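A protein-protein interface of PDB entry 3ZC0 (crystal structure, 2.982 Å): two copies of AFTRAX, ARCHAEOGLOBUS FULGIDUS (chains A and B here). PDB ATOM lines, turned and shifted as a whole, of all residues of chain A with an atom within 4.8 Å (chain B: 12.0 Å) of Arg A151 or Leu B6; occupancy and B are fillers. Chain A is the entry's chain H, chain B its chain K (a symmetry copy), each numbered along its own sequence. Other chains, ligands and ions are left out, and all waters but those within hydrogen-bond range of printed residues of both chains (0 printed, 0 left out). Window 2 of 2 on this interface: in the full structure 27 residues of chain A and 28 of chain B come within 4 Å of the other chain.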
ATOM      1  N   PHE A 100     -19.370  -1.881  21.404  1.00  0.00           N
ATOM      2  CA  PHE A 100     -20.282  -0.745  21.433  1.00  0.00           C
ATOM      3  C   PHE A 100     -20.080   0.108  20.186  1.00  0.00           C
ATOM      4  O   PHE A 100     -20.987   0.799  19.722  1.00  0.00           O
ATOM      5  CB  PHE A 100     -20.041   0.105  22.675  1.00  0.00           C
ATOM      6  CG  PHE A 100     -20.586  -0.495  23.937  1.00  0.00           C
ATOM      7  CD1 PHE A 100     -21.945  -0.643  24.119  1.00  0.00           C
ATOM      8  CD2 PHE A 100     -19.732  -0.888  24.951  1.00  0.00           C
ATOM      9  CE1 PHE A 100     -22.440  -1.180  25.277  1.00  0.00           C
ATOM     10  CE2 PHE A 100     -20.222  -1.425  26.115  1.00  0.00           C
ATOM     11  CZ  PHE A 100     -21.580  -1.571  26.276  1.00  0.00           C
ATOM     12  N   PHE A 111     -29.985   4.146  20.785  1.00  0.00           N
ATOM     13  CA  PHE A 111     -28.735   3.407  20.945  1.00  0.00           C
ATOM     14  C   PHE A 111     -28.729   2.633  22.284  1.00  0.00           C
ATOM     15  O   PHE A 111     -28.784   1.378  22.331  1.00  0.00           O
ATOM     16  CB  PHE A 111     -27.588   4.428  20.898  1.00  0.00           C
ATOM     17  CG  PHE A 111     -26.230   3.819  20.835  1.00  0.00           C
ATOM     18  CD1 PHE A 111     -25.766   3.256  19.658  1.00  0.00           C
ATOM     19  CD2 PHE A 111     -25.412   3.820  21.946  1.00  0.00           C
ATOM     20  CE1 PHE A 111     -24.510   2.692  19.594  1.00  0.00           C
ATOM     21  CE2 PHE A 111     -24.153   3.256  21.892  1.00  0.00           C
ATOM     22  CZ  PHE A 111     -23.700   2.693  20.716  1.00  0.00           C
ATOM     23  N   LEU A 112     -28.668   3.405  23.366  1.00  0.00           N
ATOM     24  CA  LEU A 112     -28.706   2.873  24.717  1.00  0.00           C
ATOM     25  C   LEU A 112     -29.780   1.780  24.897  1.00  0.00           C
ATOM     26  O   LEU A 112     -29.495   0.631  25.289  1.00  0.00           O
ATOM     27  CB  LEU A 112     -28.907   4.032  25.712  1.00  0.00           C
ATOM     28  CG  LEU A 112     -27.638   4.715  26.260  1.00  0.00           C
ATOM     29  CD1 LEU A 112     -26.404   4.356  25.468  1.00  0.00           C
ATOM     30  CD2 LEU A 112     -27.784   6.217  26.313  1.00  0.00           C
ATOM     31  N   LYS A 147     -21.315  -7.094  30.681  1.00  0.00           N
ATOM     32  CA  LYS A 147     -20.648  -5.899  30.132  1.00  0.00           C
ATOM     33  C   LYS A 147     -21.622  -4.785  29.775  1.00  0.00           C
ATOM     34  O   LYS A 147     -21.468  -3.638  30.208  1.00  0.00           O
ATOM     35  CB  LYS A 147     -19.824  -6.247  28.896  1.00  0.00           C
ATOM     36  CG  LYS A 147     -18.933  -5.096  28.423  1.00  0.00           C
ATOM     37  CD  LYS A 147     -17.944  -5.534  27.330  1.00  0.00           C
ATOM     38  CE  LYS A 147     -17.013  -6.655  27.814  1.00  0.00           C
ATOM     39  NZ  LYS A 147     -16.557  -7.574  26.716  1.00  0.00           N
ATOM     40  N   ILE A 148     -22.623  -5.143  28.977  1.00  0.00           N
ATOM     41  CA  ILE A 148     -23.697  -4.230  28.624  1.00  0.00           C
ATOM     42  C   ILE A 148     -24.308  -3.588  29.862  1.00  0.00           C
ATOM     43  O   ILE A 148     -24.520  -2.373  29.881  1.00  0.00           O
ATOM     44  CB  ILE A 148     -24.798  -4.936  27.804  1.00  0.00           C
ATOM     45  CG1 ILE A 148     -24.248  -5.383  26.444  1.00  0.00           C
ATOM     46  CG2 ILE A 148     -26.015  -4.024  27.640  1.00  0.00           C
ATOM     47  CD1 ILE A 148     -25.297  -5.983  25.518  1.00  0.00           C
ATOM     48  N   TYR A 149     -24.576  -4.389  30.900  1.00  0.00           N
ATOM     49  CA  TYR A 149     -25.165  -3.829  32.118  1.00  0.00           C
ATOM     50  C   TYR A 149     -24.233  -2.826  32.790  1.00  0.00           C
ATOM     51  O   TYR A 149     -24.622  -1.674  33.071  1.00  0.00           O
ATOM     52  CB  TYR A 149     -25.552  -4.911  33.135  1.00  0.00           C
ATOM     53  CG  TYR A 149     -26.258  -4.321  34.345  1.00  0.00           C
ATOM     54  CD1 TYR A 149     -27.623  -4.102  34.335  1.00  0.00           C
ATOM     55  CD2 TYR A 149     -25.554  -3.944  35.473  1.00  0.00           C
ATOM     56  CE1 TYR A 149     -28.271  -3.543  35.424  1.00  0.00           C
ATOM     57  CE2 TYR A 149     -26.198  -3.382  36.578  1.00  0.00           C
ATOM     58  CZ  TYR A 149     -27.556  -3.185  36.546  1.00  0.00           C
ATOM     59  OH  TYR A 149     -28.214  -2.633  37.624  1.00  0.00           O
ATOM     60  N   GLU A 150     -23.004  -3.274  33.051  1.00  0.00           N
ATOM     61  CA  GLU A 150     -22.038  -2.466  33.778  1.00  0.00           C
ATOM     62  C   GLU A 150     -21.863  -1.127  33.094  1.00  0.00           C
ATOM     63  O   GLU A 150     -21.824  -0.079  33.743  1.00  0.00           O
ATOM     64  CB  GLU A 150     -20.689  -3.176  33.856  1.00  0.00           C
ATOM     65  CG  GLU A 150     -20.651  -4.404  34.747  1.00  0.00           C
ATOM     66  CD  GLU A 150     -19.381  -5.230  34.550  1.00  0.00           C
ATOM     67  OE1 GLU A 150     -18.518  -4.838  33.724  1.00  0.00           O
ATOM     68  OE2 GLU A 150     -19.252  -6.278  35.222  1.00  0.00           O
ATOM     69  N   ARG A 151     -21.792  -1.176  31.773  1.00  0.00           N
ATOM     70  CA  ARG A 151     -21.455  -0.007  30.978  1.00  0.00           C
ATOM     71  C   ARG A 151     -22.656   0.948  30.805  1.00  0.00           C
ATOM     72  O   ARG A 151     -22.524   2.163  31.013  1.00  0.00           O
ATOM     73  CB  ARG A 151     -20.900  -0.475  29.633  1.00  0.00           C
ATOM     74  CG  ARG A 151     -19.953   0.467  28.989  1.00  0.00           C
ATOM     75  CD  ARG A 151     -18.550   0.383  29.545  1.00  0.00           C
ATOM     76  NE  ARG A 151     -17.602   0.811  28.513  1.00  0.00           N
ATOM     77  CZ  ARG A 151     -17.373   2.077  28.155  1.00  0.00           C
ATOM     78  NH1 ARG A 151     -18.004   3.093  28.751  1.00  0.00           N
ATOM     79  NH2 ARG A 151     -16.499   2.325  27.184  1.00  0.00           N
ATOM     80  N   LEU A 152     -23.820   0.403  30.437  1.00  0.00           N
ATOM     81  CA  LEU A 152     -25.034   1.206  30.324  1.00  0.00           C
ATOM     82  C   LEU A 152     -25.398   1.898  31.635  1.00  0.00           C
ATOM     83  O   LEU A 152     -25.879   3.033  31.630  1.00  0.00           O
ATOM     84  CB  LEU A 152     -26.212   0.358  29.850  1.00  0.00           C
ATOM     85  CG  LEU A 152     -26.674   0.572  28.419  1.00  0.00           C
ATOM     86  CD1 LEU A 152     -25.484   0.969  27.568  1.00  0.00           C
ATOM     87  CD2 LEU A 152     -27.352  -0.682  27.863  1.00  0.00           C
ATOM     88  N   MET A 153     -25.167   1.218  32.760  1.00  0.00           N
ATOM     89  CA  MET A 153     -25.595   1.750  34.063  1.00  0.00           C
ATOM     90  C   MET A 153     -25.055   3.148  34.337  1.00  0.00           C
ATOM     91  O   MET A 153     -25.627   3.903  35.136  1.00  0.00           O
ATOM     92  CB  MET A 153     -25.205   0.807  35.199  1.00  0.00           C
ATOM     93  CG  MET A 153     -26.275  -0.208  35.560  1.00  0.00           C
ATOM     94  SD  MET A 153     -27.739   0.514  36.325  1.00  0.00           S
ATOM     95  CE  MET A 153     -27.007   1.455  37.655  1.00  0.00           C
ATOM     96  N   GLU A 154     -23.956   3.483  33.661  1.00  0.00           N
ATOM     97  CA  GLU A 154     -23.316   4.773  33.821  1.00  0.00           C
ATOM     98  C   GLU A 154     -24.224   5.882  33.312  1.00  0.00           C
ATOM     99  O   GLU A 154     -24.180   7.011  33.811  1.00  0.00           O
ATOM    100  CB  GLU A 154     -21.968   4.795  33.097  1.00  0.00           C
ATOM    101  CG  GLU A 154     -20.833   4.152  33.885  1.00  0.00           C
ATOM    102  CD  GLU A 154     -19.743   3.589  32.983  1.00  0.00           C
ATOM    103  OE1 GLU A 154     -19.890   3.700  31.739  1.00  0.00           O
ATOM    104  OE2 GLU A 154     -18.748   3.036  33.512  1.00  0.00           O
ATOM    105  N   PHE A 155     -25.067   5.558  32.333  1.00  0.00           N
ATOM    106  CA  PHE A 155     -25.945   6.567  31.740  1.00  0.00           C
ATOM    107  C   PHE A 155     -27.223   6.795  32.528  1.00  0.00           C
ATOM    108  O   PHE A 155     -28.089   7.562  32.099  1.00  0.00           O
ATOM    109  CB  PHE A 155     -26.288   6.229  30.294  1.00  0.00           C
ATOM    110  CG  PHE A 155     -25.127   6.351  29.348  1.00  0.00           C
ATOM    111  CD1 PHE A 155     -24.105   5.422  29.355  1.00  0.00           C
ATOM    112  CD2 PHE A 155     -25.071   7.389  28.429  1.00  0.00           C
ATOM    113  CE1 PHE A 155     -23.048   5.533  28.462  1.00  0.00           C
ATOM    114  CE2 PHE A 155     -24.010   7.506  27.536  1.00  0.00           C
ATOM    115  CZ  PHE A 155     -23.003   6.575  27.549  1.00  0.00           C
ATOM    116  N   MET B   4     -15.147   7.044  19.909  1.00  0.00           N
ATOM    117  CA  MET B   4     -15.792   5.948  20.635  1.00  0.00           C
ATOM    118  C   MET B   4     -17.254   6.237  21.020  1.00  0.00           C
ATOM    119  O   MET B   4     -17.533   7.059  21.905  1.00  0.00           O
ATOM    120  CB  MET B   4     -14.972   5.552  21.858  1.00  0.00           C
ATOM    121  CG  MET B   4     -13.806   4.635  21.536  1.00  0.00           C
ATOM    122  SD  MET B   4     -12.954   4.072  23.028  1.00  0.00           S
ATOM    123  CE  MET B   4     -12.476   5.649  23.738  1.00  0.00           C
ATOM    124  N   ARG B   5     -18.163   5.516  20.354  1.00  0.00           N
ATOM    125  CA  ARG B   5     -19.616   5.779  20.336  1.00  0.00           C
ATOM    126  C   ARG B   5     -20.286   6.160  21.665  1.00  0.00           C
ATOM    127  O   ARG B   5     -21.075   7.106  21.710  1.00  0.00           O
ATOM    128  CB  ARG B   5     -20.362   4.607  19.672  1.00  0.00           C
ATOM    129  CG  ARG B   5     -20.845   4.898  18.245  1.00  0.00           C
ATOM    130  CD  ARG B   5     -21.785   6.113  18.228  1.00  0.00           C
ATOM    131  NE  ARG B   5     -23.132   5.796  17.752  1.00  0.00           N
ATOM    132  CZ  ARG B   5     -24.198   6.563  17.958  1.00  0.00           C
ATOM    133  NH1 ARG B   5     -24.088   7.694  18.640  1.00  0.00           N
ATOM    134  NH2 ARG B   5     -25.374   6.192  17.485  1.00  0.00           N
ATOM    135  N   LEU B   6     -19.977   5.429  22.732  1.00  0.00           N
ATOM    136  CA  LEU B   6     -20.501   5.749  24.059  1.00  0.00           C
ATOM    137  C   LEU B   6     -20.194   7.181  24.504  1.00  0.00           C
ATOM    138  O   LEU B   6     -20.994   7.816  25.207  1.00  0.00           O
ATOM    139  CB  LEU B   6     -19.977   4.752  25.089  1.00  0.00           C
ATOM    140  CG  LEU B   6     -20.659   3.385  24.968  1.00  0.00           C
ATOM    141  CD1 LEU B   6     -20.162   2.458  26.042  1.00  0.00           C
ATOM    142  CD2 LEU B   6     -22.182   3.528  25.050  1.00  0.00           C
ATOM    143  N   GLU B   7     -19.043   7.689  24.081  1.00  0.00           N
ATOM    144  CA  GLU B   7     -18.643   9.035  24.445  1.00  0.00           C
ATOM    145  C   GLU B   7     -19.385  10.051  23.592  1.00  0.00           C
ATOM    146  O   GLU B   7     -19.686  11.160  24.051  1.00  0.00           O
ATOM    147  CB  GLU B   7     -17.127   9.200  24.338  1.00  0.00           C
ATOM    148  CG  GLU B   7     -16.340   8.256  25.249  1.00  0.00           C
ATOM    149  CD  GLU B   7     -16.764   8.356  26.709  1.00  0.00           C
ATOM    150  OE1 GLU B   7     -17.024   9.493  27.182  1.00  0.00           O
ATOM    151  OE2 GLU B   7     -16.838   7.293  27.377  1.00  0.00           O
ATOM    152  N   GLU B   8     -19.703   9.666  22.359  1.00  0.00           N
ATOM    153  CA  GLU B   8     -20.540  10.502  21.493  1.00  0.00           C
ATOM    154  C   GLU B   8     -21.962  10.632  22.080  1.00  0.00           C
ATOM    155  O   GLU B   8     -22.570  11.718  22.072  1.00  0.00           O
ATOM    156  CB  GLU B   8     -20.565   9.936  20.064  1.00  0.00           C
ATOM    157  N   CYS B   9     -22.472   9.512  22.594  1.00  0.00           N
ATOM    158  CA  CYS B   9     -23.713   9.484  23.367  1.00  0.00           C
ATOM    159  C   CYS B   9     -23.658  10.442  24.541  1.00  0.00           C
ATOM    160  O   CYS B   9     -24.418  11.400  24.570  1.00  0.00           O
ATOM    161  CB  CYS B   9     -24.002   8.084  23.903  1.00  0.00           C
ATOM    162  SG  CYS B   9     -24.830   6.994  22.753  1.00  0.00           S
ATOM    163  N   ARG B  10     -22.774  10.159  25.505  1.00  0.00           N
ATOM    164  CA  ARG B  10     -22.568  11.018  26.683  1.00  0.00           C
ATOM    165  C   ARG B  10     -22.500  12.518  26.320  1.00  0.00           C
ATOM    166  O   ARG B  10     -23.187  13.354  26.932  1.00  0.00           O
ATOM    167  CB  ARG B  10     -21.306  10.570  27.459  1.00  0.00           C
ATOM    168  CG  ARG B  10     -20.836  11.478  28.626  1.00  0.00           C
ATOM    169  CD  ARG B  10     -21.493  11.157  29.979  1.00  0.00           C
ATOM    170  NE  ARG B  10     -21.443   9.727  30.290  1.00  0.00           N
ATOM    171  CZ  ARG B  10     -21.897   9.167  31.412  1.00  0.00           C
ATOM    172  NH1 ARG B  10     -22.438   9.910  32.378  1.00  0.00           N
ATOM    173  NH2 ARG B  10     -21.802   7.850  31.565  1.00  0.00           N
ATOM    174  N   LYS B  11     -21.690  12.846  25.315  1.00  0.00           N
ATOM    175  CA  LYS B  11     -21.575  14.221  24.844  1.00  0.00           C
ATOM    176  C   LYS B  11     -22.951  14.764  24.462  1.00  0.00           C
ATOM    177  O   LYS B  11     -23.462  15.718  25.079  1.00  0.00           O
ATOM    178  CB  LYS B  11     -20.627  14.300  23.642  1.00  0.00           C
ATOM    179  N   ARG B  12     -23.558  14.128  23.462  1.00  0.00           N
ATOM    180  CA  ARG B  12     -24.846  14.571  22.944  1.00  0.00           C
ATOM    181  C   ARG B  12     -25.946  14.688  24.018  1.00  0.00           C
ATOM    182  O   ARG B  12     -26.780  15.593  23.960  1.00  0.00           O
ATOM    183  CB  ARG B  12     -25.283  13.665  21.794  1.00  0.00           C
ATOM    184  CG  ARG B  12     -26.609  14.074  21.151  1.00  0.00           C
ATOM    185  CD  ARG B  12     -26.608  15.523  20.666  1.00  0.00           C
ATOM    186  NE  ARG B  12     -27.641  15.745  19.657  1.00  0.00           N
ATOM    187  CZ  ARG B  12     -27.921  16.924  19.108  1.00  0.00           C
ATOM    188  NH1 ARG B  12     -27.251  18.013  19.468  1.00  0.00           N
ATOM    189  NH2 ARG B  12     -28.881  17.016  18.199  1.00  0.00           N
ATOM    190  N   LEU B  13     -25.928  13.791  25.000  1.00  0.00           N
ATOM    191  CA  LEU B  13     -26.872  13.851  26.112  1.00  0.00           C
ATOM    192  C   LEU B  13     -26.615  15.031  27.042  1.00  0.00           C
ATOM    193  O   LEU B  13     -27.568  15.640  27.538  1.00  0.00           O
ATOM    194  CB  LEU B  13     -26.887  12.544  26.909  1.00  0.00           C
ATOM    195  CG  LEU B  13     -27.649  11.383  26.274  1.00  0.00           C
ATOM    196  CD1 LEU B  13     -27.545  10.166  27.157  1.00  0.00           C
ATOM    197  CD2 LEU B  13     -29.107  11.768  26.068  1.00  0.00           C
ATOM    198  N   GLU B  14     -25.345  15.358  27.287  1.00  0.00           N
ATOM    199  CA  GLU B  14     -25.045  16.537  28.107  1.00  0.00           C
ATOM    200  C   GLU B  14     -25.509  17.817  27.385  1.00  0.00           C
ATOM    201  O   GLU B  14     -26.175  18.696  27.983  1.00  0.00           O
ATOM    202  CB  GLU B  14     -23.557  16.607  28.444  1.00  0.00           C
ATOM    203  CG  GLU B  14     -23.082  15.539  29.398  1.00  0.00           C
ATOM    204  CD  GLU B  14     -21.569  15.429  29.439  1.00  0.00           C
ATOM    205  OE1 GLU B  14     -20.897  16.345  28.918  1.00  0.00           O
ATOM    206  OE2 GLU B  14     -21.059  14.424  29.987  1.00  0.00           O
ATOM    207  N   GLU B  15     -25.159  17.898  26.096  1.00  0.00           N
ATOM    208  CA  GLU B  15     -25.641  18.962  25.219  1.00  0.00           C
ATOM    209  C   GLU B  15     -27.165  19.120  25.320  1.00  0.00           C
ATOM    210  O   GLU B  15     -27.678  20.199  25.637  1.00  0.00           O
ATOM    211  CB  GLU B  15     -25.253  18.666  23.764  1.00  0.00           C
ATOM    212  CG  GLU B  15     -23.779  18.864  23.421  1.00  0.00           C
ATOM    213  CD  GLU B  15     -23.526  18.816  21.921  1.00  0.00           C
ATOM    214  OE1 GLU B  15     -24.189  18.011  21.239  1.00  0.00           O
ATOM    215  OE2 GLU B  15     -22.672  19.579  21.420  1.00  0.00           O
ATOM    216  N   LEU B  16     -27.878  18.030  25.059  1.00  0.00           N
ATOM    217  CA  LEU B  16     -29.326  18.035  25.098  1.00  0.00           C
ATOM    218  C   LEU B  16     -29.906  18.451  26.450  1.00  0.00           C
ATOM    219  O   LEU B  16     -30.843  19.249  26.487  1.00  0.00           O
ATOM    220  CB  LEU B  16     -29.881  16.675  24.649  1.00  0.00           C
ATOM    221  CG  LEU B  16     -29.969  16.496  23.124  1.00  0.00           C
ATOM    222  CD1 LEU B  16     -30.192  15.038  22.705  1.00  0.00           C
ATOM    223  CD2 LEU B  16     -31.058  17.399  22.543  1.00  0.00           C
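No position is printed for both chains.
Of the 11 pairs that touch across the chains among the printed residues, none has its exchanged pair printed and touching as well.
The guanidinium group (NH2) of Arg B10 sits at hydrogen-bond distance from the backbone carbonyl oxygen (O) of Glu A154, 3.4 Å away.
Of the 12 printed residues of chain A, 5 touch a printed residue of chain B.
Along chain A the printed residues that touch a printed residue of chain B span positions 100 to 155.
Of the 13 printed residues of chain B, 5 touch a printed residue of chain A.
Hydrophobic or aromatic side chains of chain B within 4 Å of the printed part of chain A: Leu B6 and Leu B13.
Among the printed residues, no Asp or Glu carboxylate lies within 4 Å of a Lys or Arg side-chain nitrogen of the other chain.
Among the printed residues, pairs that only touch across the chains: Phe A155 with Leu B6, Phe A111 with Cys B9, Arg A151 with Leu B6, Phe A100 with Leu B6, Phe A155 with Arg B10, Phe A111 with Arg B5, Phe A155 with Cys B9, Phe A111 with Leu B6, Phe A100 with Arg B5 and Phe A155 with Leu B13.
Of the printed residues of chain B, Phe A111 touches Arg B5 (3.7 Å), Leu B6 (3.7 Å) and Cys B9 (3.3 Å).
No residue of chain B comes within 4 Å of Leu A112.
Of chain B, only Leu B6 comes within 4 Å of Arg A151.
No residue of chain B comes within 4 Å of Leu A152.
Printed residues of chain B within 4 Å of Glu A154: Arg B10.
Of chain B, only Leu B6, Cys B9, Arg B10 and Leu B13 come within 4 Å of Phe A155.
Leu B6 touches just these residues of chain A: Phe A100, Phe A111, Arg A151 and Phe A155.
Glu B8 touches none of the printed residues of chain A.
Printed residues of chain A within 4 Å of Cys B9: Phe A111 and Phe A155.
Of the printed residues of chain A, Arg B10 touches Glu A154 (3.4 Å) and Phe A155 (3.6 Å).
Arg B12 touches none of the printed residues of chain A.
Of the printed residues of chain A, Leu B13 touches Phe A155.
The nearest residue of chain A that does not touch Leu B6 is Leu A112 (4.3 Å).
The guanidinium group of Arg A151 lies within salt-bridge range of the side-chain carboxylate of Glu A154 (3.6 Å).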
